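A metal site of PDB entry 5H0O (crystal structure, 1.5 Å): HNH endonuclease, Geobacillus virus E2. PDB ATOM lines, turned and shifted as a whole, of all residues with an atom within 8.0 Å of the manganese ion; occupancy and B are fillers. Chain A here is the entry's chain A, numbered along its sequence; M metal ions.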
ATOM      1  N   LEU A  75     -13.743  -5.751   3.618  1.00  0.00           N
ATOM      2  CA  LEU A  75     -12.931  -5.845   4.835  1.00  0.00           C
ATOM      3  C   LEU A  75     -13.646  -6.676   5.883  1.00  0.00           C
ATOM      4  O   LEU A  75     -14.864  -6.550   6.064  1.00  0.00           O
ATOM      5  CB  LEU A  75     -12.612  -4.472   5.394  1.00  0.00           C
ATOM      6  CG  LEU A  75     -11.722  -3.596   4.506  1.00  0.00           C
ATOM      7  CD1 LEU A  75     -11.449  -2.278   5.224  1.00  0.00           C
ATOM      8  CD2 LEU A  75     -10.422  -4.328   4.161  1.00  0.00           C
ATOM      9  N   CYS A  76     -12.883  -7.505   6.607  1.00  0.00           N
ATOM     10  CA  CYS A  76     -13.434  -8.278   7.708  1.00  0.00           C
ATOM     11  C   CYS A  76     -13.894  -7.338   8.813  1.00  0.00           C
ATOM     12  O   CYS A  76     -13.103  -6.533   9.320  1.00  0.00           O
ATOM     13  CB  CYS A  76     -12.387  -9.236   8.268  1.00  0.00           C
ATOM     14  SG  CYS A  76     -12.999 -10.095   9.736  1.00  0.00           S
ATOM     15  N   GLN A  77     -15.151  -7.461   9.212  1.00  0.00           N
ATOM     16  CA  GLN A  77     -15.738  -6.551  10.178  1.00  0.00           C
ATOM     17  C   GLN A  77     -15.295  -6.829  11.603  1.00  0.00           C
ATOM     18  O   GLN A  77     -15.191  -5.902  12.401  1.00  0.00           O
ATOM     19  CB  GLN A  77     -17.260  -6.613  10.064  1.00  0.00           C
ATOM     20  CG  GLN A  77     -17.768  -6.115   8.716  1.00  0.00           C
ATOM     21  CD  GLN A  77     -17.347  -4.686   8.449  1.00  0.00           C
ATOM     22  OE1 GLN A  77     -17.888  -3.739   9.052  1.00  0.00           O
ATOM     23  NE2 GLN A  77     -16.370  -4.499   7.570  1.00  0.00           N
ATOM     24  N   HIS A  78     -15.004  -8.084  11.931  1.00  0.00           N
ATOM     25  CA  HIS A  78     -14.510  -8.388  13.269  1.00  0.00           C
ATOM     26  C   HIS A  78     -13.083  -7.880  13.416  1.00  0.00           C
ATOM     27  O   HIS A  78     -12.738  -7.271  14.433  1.00  0.00           O
ATOM     28  CB  HIS A  78     -14.577  -9.876  13.567  1.00  0.00           C
ATOM     29  CG  HIS A  78     -15.959 -10.413  13.713  1.00  0.00           C
ATOM     30  ND1 HIS A  78     -16.212 -11.704  14.105  1.00  0.00           N
ATOM     31  CD2 HIS A  78     -17.174  -9.829  13.521  1.00  0.00           C
ATOM     32  CE1 HIS A  78     -17.513 -11.909  14.155  1.00  0.00           C
ATOM     33  NE2 HIS A  78     -18.112 -10.783  13.800  1.00  0.00           N
ATOM     34  N   CYS A  79     -12.251  -8.105  12.397  1.00  0.00           N
ATOM     35  CA  CYS A  79     -10.908  -7.544  12.401  1.00  0.00           C
ATOM     36  C   CYS A  79     -10.941  -6.027  12.560  1.00  0.00           C
ATOM     37  O   CYS A  79     -10.187  -5.462  13.350  1.00  0.00           O
ATOM     38  CB  CYS A  79     -10.160  -7.947  11.127  1.00  0.00           C
ATOM     39  SG  CYS A  79      -9.446  -9.631  11.178  1.00  0.00           S
ATOM     40  N   LEU A  80     -11.832  -5.361  11.833  1.00  0.00           N
ATOM     41  CA  LEU A  80     -11.895  -3.899  11.889  1.00  0.00           C
ATOM     42  C   LEU A  80     -12.181  -3.430  13.316  1.00  0.00           C
ATOM     43  O   LEU A  80     -11.560  -2.471  13.791  1.00  0.00           O
ATOM     44  CB  LEU A  80     -12.947  -3.391  10.906  1.00  0.00           C
ATOM     45  CG  LEU A  80     -12.894  -1.930  10.465  1.00  0.00           C
ATOM     46  CD1 LEU A  80     -11.548  -1.565   9.879  1.00  0.00           C
ATOM     47  CD2 LEU A  80     -13.997  -1.706   9.440  1.00  0.00           C
ATOM     48  N   GLU A  82     -11.287  -4.902  15.924  1.00  0.00           N
ATOM     49  CA  GLU A  82     -10.053  -5.171  16.657  1.00  0.00           C
ATOM     50  C   GLU A  82      -8.865  -4.360  16.115  1.00  0.00           C
ATOM     51  O   GLU A  82      -7.713  -4.654  16.457  1.00  0.00           O
ATOM     52  CB  GLU A  82      -9.749  -6.686  16.614  1.00  0.00           C
ATOM     53  CG  GLU A  82     -10.846  -7.531  17.286  1.00  0.00           C
ATOM     54  CD  GLU A  82     -10.711  -9.042  17.061  1.00  0.00           C
ATOM     55  OE1 GLU A  82     -10.494  -9.474  15.914  1.00  0.00           O
ATOM     56  OE2 GLU A  82     -10.840  -9.801  18.048  1.00  0.00           O
ATOM     57  N   LYS A  84      -7.668  -4.101  13.000  1.00  0.00           N
ATOM     58  CA  LYS A  84      -6.902  -4.853  12.029  1.00  0.00           C
ATOM     59  C   LYS A  84      -7.537  -4.812  10.666  1.00  0.00           C
ATOM     60  O   LYS A  84      -8.722  -4.758  10.550  1.00  0.00           O
ATOM     61  CB  LYS A  84      -6.816  -6.312  12.429  1.00  0.00           C
ATOM     62  CG  LYS A  84      -6.075  -6.609  13.713  1.00  0.00           C
ATOM     63  CD  LYS A  84      -6.096  -8.113  13.973  1.00  0.00           C
ATOM     64  CE  LYS A  84      -5.714  -8.921  12.716  1.00  0.00           C
ATOM     65  NZ  LYS A  84      -5.995 -10.387  12.766  1.00  0.00           N
ATOM     66  N   ILE A  85      -6.715  -4.814   9.637  1.00  0.00           N
ATOM     67  CA  ILE A  85      -7.175  -4.777   8.259  1.00  0.00           C
ATOM     68  C   ILE A  85      -6.945  -6.155   7.652  1.00  0.00           C
ATOM     69  O   ILE A  85      -5.788  -6.597   7.499  1.00  0.00           O
ATOM     70  CB  ILE A  85      -6.431  -3.701   7.433  1.00  0.00           C
ATOM     71  CG1 ILE A  85      -6.617  -2.308   8.052  1.00  0.00           C
ATOM     72  CG2 ILE A  85      -6.925  -3.699   6.001  1.00  0.00           C
ATOM     73  CD1 ILE A  85      -8.048  -1.839   8.161  1.00  0.00           C
ATOM     74  N   THR A  86      -8.032  -6.830   7.306  1.00  0.00           N
ATOM     75  CA  THR A  86      -7.981  -8.163   6.720  1.00  0.00           C
ATOM     76  C   THR A  86      -9.042  -8.279   5.665  1.00  0.00           C
ATOM     77  O   THR A  86     -10.197  -7.920   5.924  1.00  0.00           O
ATOM     78  CB  THR A  86      -8.187  -9.266   7.776  1.00  0.00           C
ATOM     79  OG1 THR A  86      -7.358  -9.019   8.921  1.00  0.00           O
ATOM     80  CG2 THR A  86      -7.879 -10.635   7.184  1.00  0.00           C
ATOM     81  N   ARG A  87      -8.689  -8.800   4.494  1.00  0.00           N
ATOM     82  CA  ARG A  87      -9.663  -9.008   3.430  1.00  0.00           C
ATOM     83  C   ARG A  87     -10.694 -10.051   3.855  1.00  0.00           C
ATOM     84  O   ARG A  87     -10.354 -11.113   4.391  1.00  0.00           O
ATOM     85  CB  ARG A  87      -8.979  -9.443   2.132  1.00  0.00           C
ATOM     86  CG  ARG A  87      -9.962  -9.629   0.984  1.00  0.00           C
ATOM     87  CD  ARG A  87      -9.275  -9.569  -0.366  1.00  0.00           C
ATOM     88  NE  ARG A  87     -10.222  -9.770  -1.466  1.00  0.00           N
ATOM     89  CZ  ARG A  87     -10.905  -8.812  -2.075  1.00  0.00           C
ATOM     90  NH1 ARG A  87     -10.769  -7.542  -1.698  1.00  0.00           N
ATOM     91  NH2 ARG A  87     -11.734  -9.111  -3.065  1.00  0.00           N
ATOM     92  N   ALA A  88     -11.956  -9.733   3.621  1.00  0.00           N
ATOM     93  CA  ALA A  88     -13.034 -10.677   3.875  1.00  0.00           C
ATOM     94  C   ALA A  88     -13.114 -11.695   2.748  1.00  0.00           C
ATOM     95  O   ALA A  88     -12.915 -11.357   1.573  1.00  0.00           O
ATOM     96  CB  ALA A  88     -14.344  -9.932   4.011  1.00  0.00           C
ATOM     97  N   SER A 112     -19.264  -9.350   6.686  1.00  0.00           N
ATOM     98  CA  SER A 112     -18.116  -9.814   5.920  1.00  0.00           C
ATOM     99  C   SER A 112     -17.019 -10.228   6.898  1.00  0.00           C
ATOM    100  O   SER A 112     -16.628  -9.443   7.768  1.00  0.00           O
ATOM    101  CB  SER A 112     -17.615  -8.703   5.001  1.00  0.00           C
ATOM    102  OG  SER A 112     -18.642  -8.240   4.137  1.00  0.00           O
ATOM    103  N   LEU A 113     -16.492 -11.440   6.726  1.00  0.00           N
ATOM    104  CA  LEU A 113     -15.478 -11.973   7.624  1.00  0.00           C
ATOM    105  C   LEU A 113     -14.304 -12.581   6.856  1.00  0.00           C
ATOM    106  O   LEU A 113     -14.476 -13.122   5.762  1.00  0.00           O
ATOM    107  CB  LEU A 113     -16.040 -13.045   8.569  1.00  0.00           C
ATOM    108  CG  LEU A 113     -17.203 -12.662   9.473  1.00  0.00           C
ATOM    109  CD1 LEU A 113     -17.645 -13.890  10.236  1.00  0.00           C
ATOM    110  CD2 LEU A 113     -16.818 -11.543  10.420  1.00  0.00           C
ATOM    111  N   CYS A 114     -13.127 -12.508   7.467  1.00  0.00           N
ATOM    112  CA  CYS A 114     -11.986 -13.317   7.040  1.00  0.00           C
ATOM    113  C   CYS A 114     -12.155 -14.753   7.535  1.00  0.00           C
ATOM    114  O   CYS A 114     -13.022 -15.045   8.346  1.00  0.00           O
ATOM    115  CB  CYS A 114     -10.680 -12.716   7.570  1.00  0.00           C
ATOM    116  SG  CYS A 114     -10.409 -12.923   9.356  1.00  0.00           S
ATOM    117  N   GLN A 115     -11.295 -15.654   7.060  1.00  0.00           N
ATOM    118  CA  GLN A 115     -11.409 -17.056   7.459  1.00  0.00           C
ATOM    119  C   GLN A 115     -11.213 -17.239   8.957  1.00  0.00           C
ATOM    120  O   GLN A 115     -11.943 -17.993   9.586  1.00  0.00           O
ATOM    121  CB  GLN A 115     -10.416 -17.933   6.720  1.00  0.00           C
ATOM    122  CG  GLN A 115     -10.491 -19.371   7.197  1.00  0.00           C
ATOM    123  CD  GLN A 115      -9.504 -20.278   6.538  1.00  0.00           C
ATOM    124  OE1 GLN A 115      -9.089 -20.031   5.421  1.00  0.00           O
ATOM    125  NE2 GLN A 115      -9.112 -21.338   7.228  1.00  0.00           N
ATOM    126  N   ALA A 116     -10.209 -16.576   9.530  1.00  0.00           N
ATOM    127  CA  ALA A 116      -9.934 -16.750  10.940  1.00  0.00           C
ATOM    128  C   ALA A 116     -11.161 -16.346  11.766  1.00  0.00           C
ATOM    129  O   ALA A 116     -11.537 -17.051  12.709  1.00  0.00           O
ATOM    130  CB  ALA A 116      -8.703 -15.975  11.376  1.00  0.00           C
ATOM    131  N   CYS A 117     -11.790 -15.236  11.404  1.00  0.00           N
ATOM    132  CA  CYS A 117     -12.959 -14.789  12.156  1.00  0.00           C
ATOM    133  C   CYS A 117     -14.178 -15.658  11.889  1.00  0.00           C
ATOM    134  O   CYS A 117     -14.991 -15.878  12.802  1.00  0.00           O
ATOM    135  CB  CYS A 117     -13.248 -13.323  11.867  1.00  0.00           C
ATOM    136  SG  CYS A 117     -11.956 -12.236  12.525  1.00  0.00           S
ATOM    137  N   HIS A 118     -14.331 -16.160  10.674  1.00  0.00           N
ATOM    138  CA  HIS A 118     -15.396 -17.120  10.394  1.00  0.00           C
ATOM    139  C   HIS A 118     -15.220 -18.405  11.205  1.00  0.00           C
ATOM    140  O   HIS A 118     -16.175 -18.885  11.820  1.00  0.00           O
ATOM    141  CB  HIS A 118     -15.439 -17.432   8.896  1.00  0.00           C
ATOM    142  CG  HIS A 118     -16.545 -18.366   8.516  1.00  0.00           C
ATOM    143  ND1 HIS A 118     -16.330 -19.530   7.832  1.00  0.00           N
ATOM    144  CD2 HIS A 118     -17.886 -18.284   8.714  1.00  0.00           C
ATOM    145  CE1 HIS A 118     -17.480 -20.146   7.628  1.00  0.00           C
ATOM    146  NE2 HIS A 118     -18.442 -19.413   8.167  1.00  0.00           N
ATOM    147  N   ARG A 120     -13.536 -18.746  14.015  1.00  0.00           N
ATOM    148  CA  ARG A 120     -13.786 -18.403  15.413  1.00  0.00           C
ATOM    149  C   ARG A 120     -15.278 -18.331  15.693  1.00  0.00           C
ATOM    150  O   ARG A 120     -15.767 -18.879  16.688  1.00  0.00           O
ATOM    151  CB  ARG A 120     -13.093 -17.079  15.765  1.00  0.00           C
ATOM    152  CG  ARG A 120     -13.469 -16.526  17.135  1.00  0.00           C
ATOM    153  CD  ARG A 120     -12.629 -15.333  17.534  1.00  0.00           C
ATOM    154  NE  ARG A 120     -12.761 -14.195  16.629  1.00  0.00           N
ATOM    155  CZ  ARG A 120     -12.189 -13.014  16.819  1.00  0.00           C
ATOM    156  NH1 ARG A 120     -11.436 -12.806  17.899  1.00  0.00           N
ATOM    157  NH2 ARG A 120     -12.346 -12.035  15.926  1.00  0.00           N
HETATM  158 MN    MN M   1     -11.133 -11.140  10.654  1.00  0.00          MN
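The manganese ion is bound by the side-chain sulfur (SG) of Cys 117 (2.3 Å), the side-chain sulfur (SG) of Cys 114 (2.3 Å), the side-chain sulfur (SG) of Cys 79 (2.3 Å) and the side-chain sulfur (SG) of Cys 76 (2.3 Å).
The manganese ion has four donor atoms within binding distance.
The side-chain sulfur (SG) of Cys 117 sits close to the guanidinium group (NH2) of Arg 120 (3.4 Å).
SG of Cys 114 sits close to N of Ala 116, at 3.7 Å.
SG of Cys 79 sits close to OG1 of Thr 86, at 3.1 Å.
The backbone carbonyl oxygen of Cys 79 is in hydrogen-bond range of the backbone NH of Lys 84, at 2.9 Å.
O of Thr 86 is in hydrogen-bond range of N of Cys 76 (2.8 Å).
The backbone NH (N) of His 78 sits close to the side-chain sulfur (SG) of Cys 76, at 3.6 Å.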
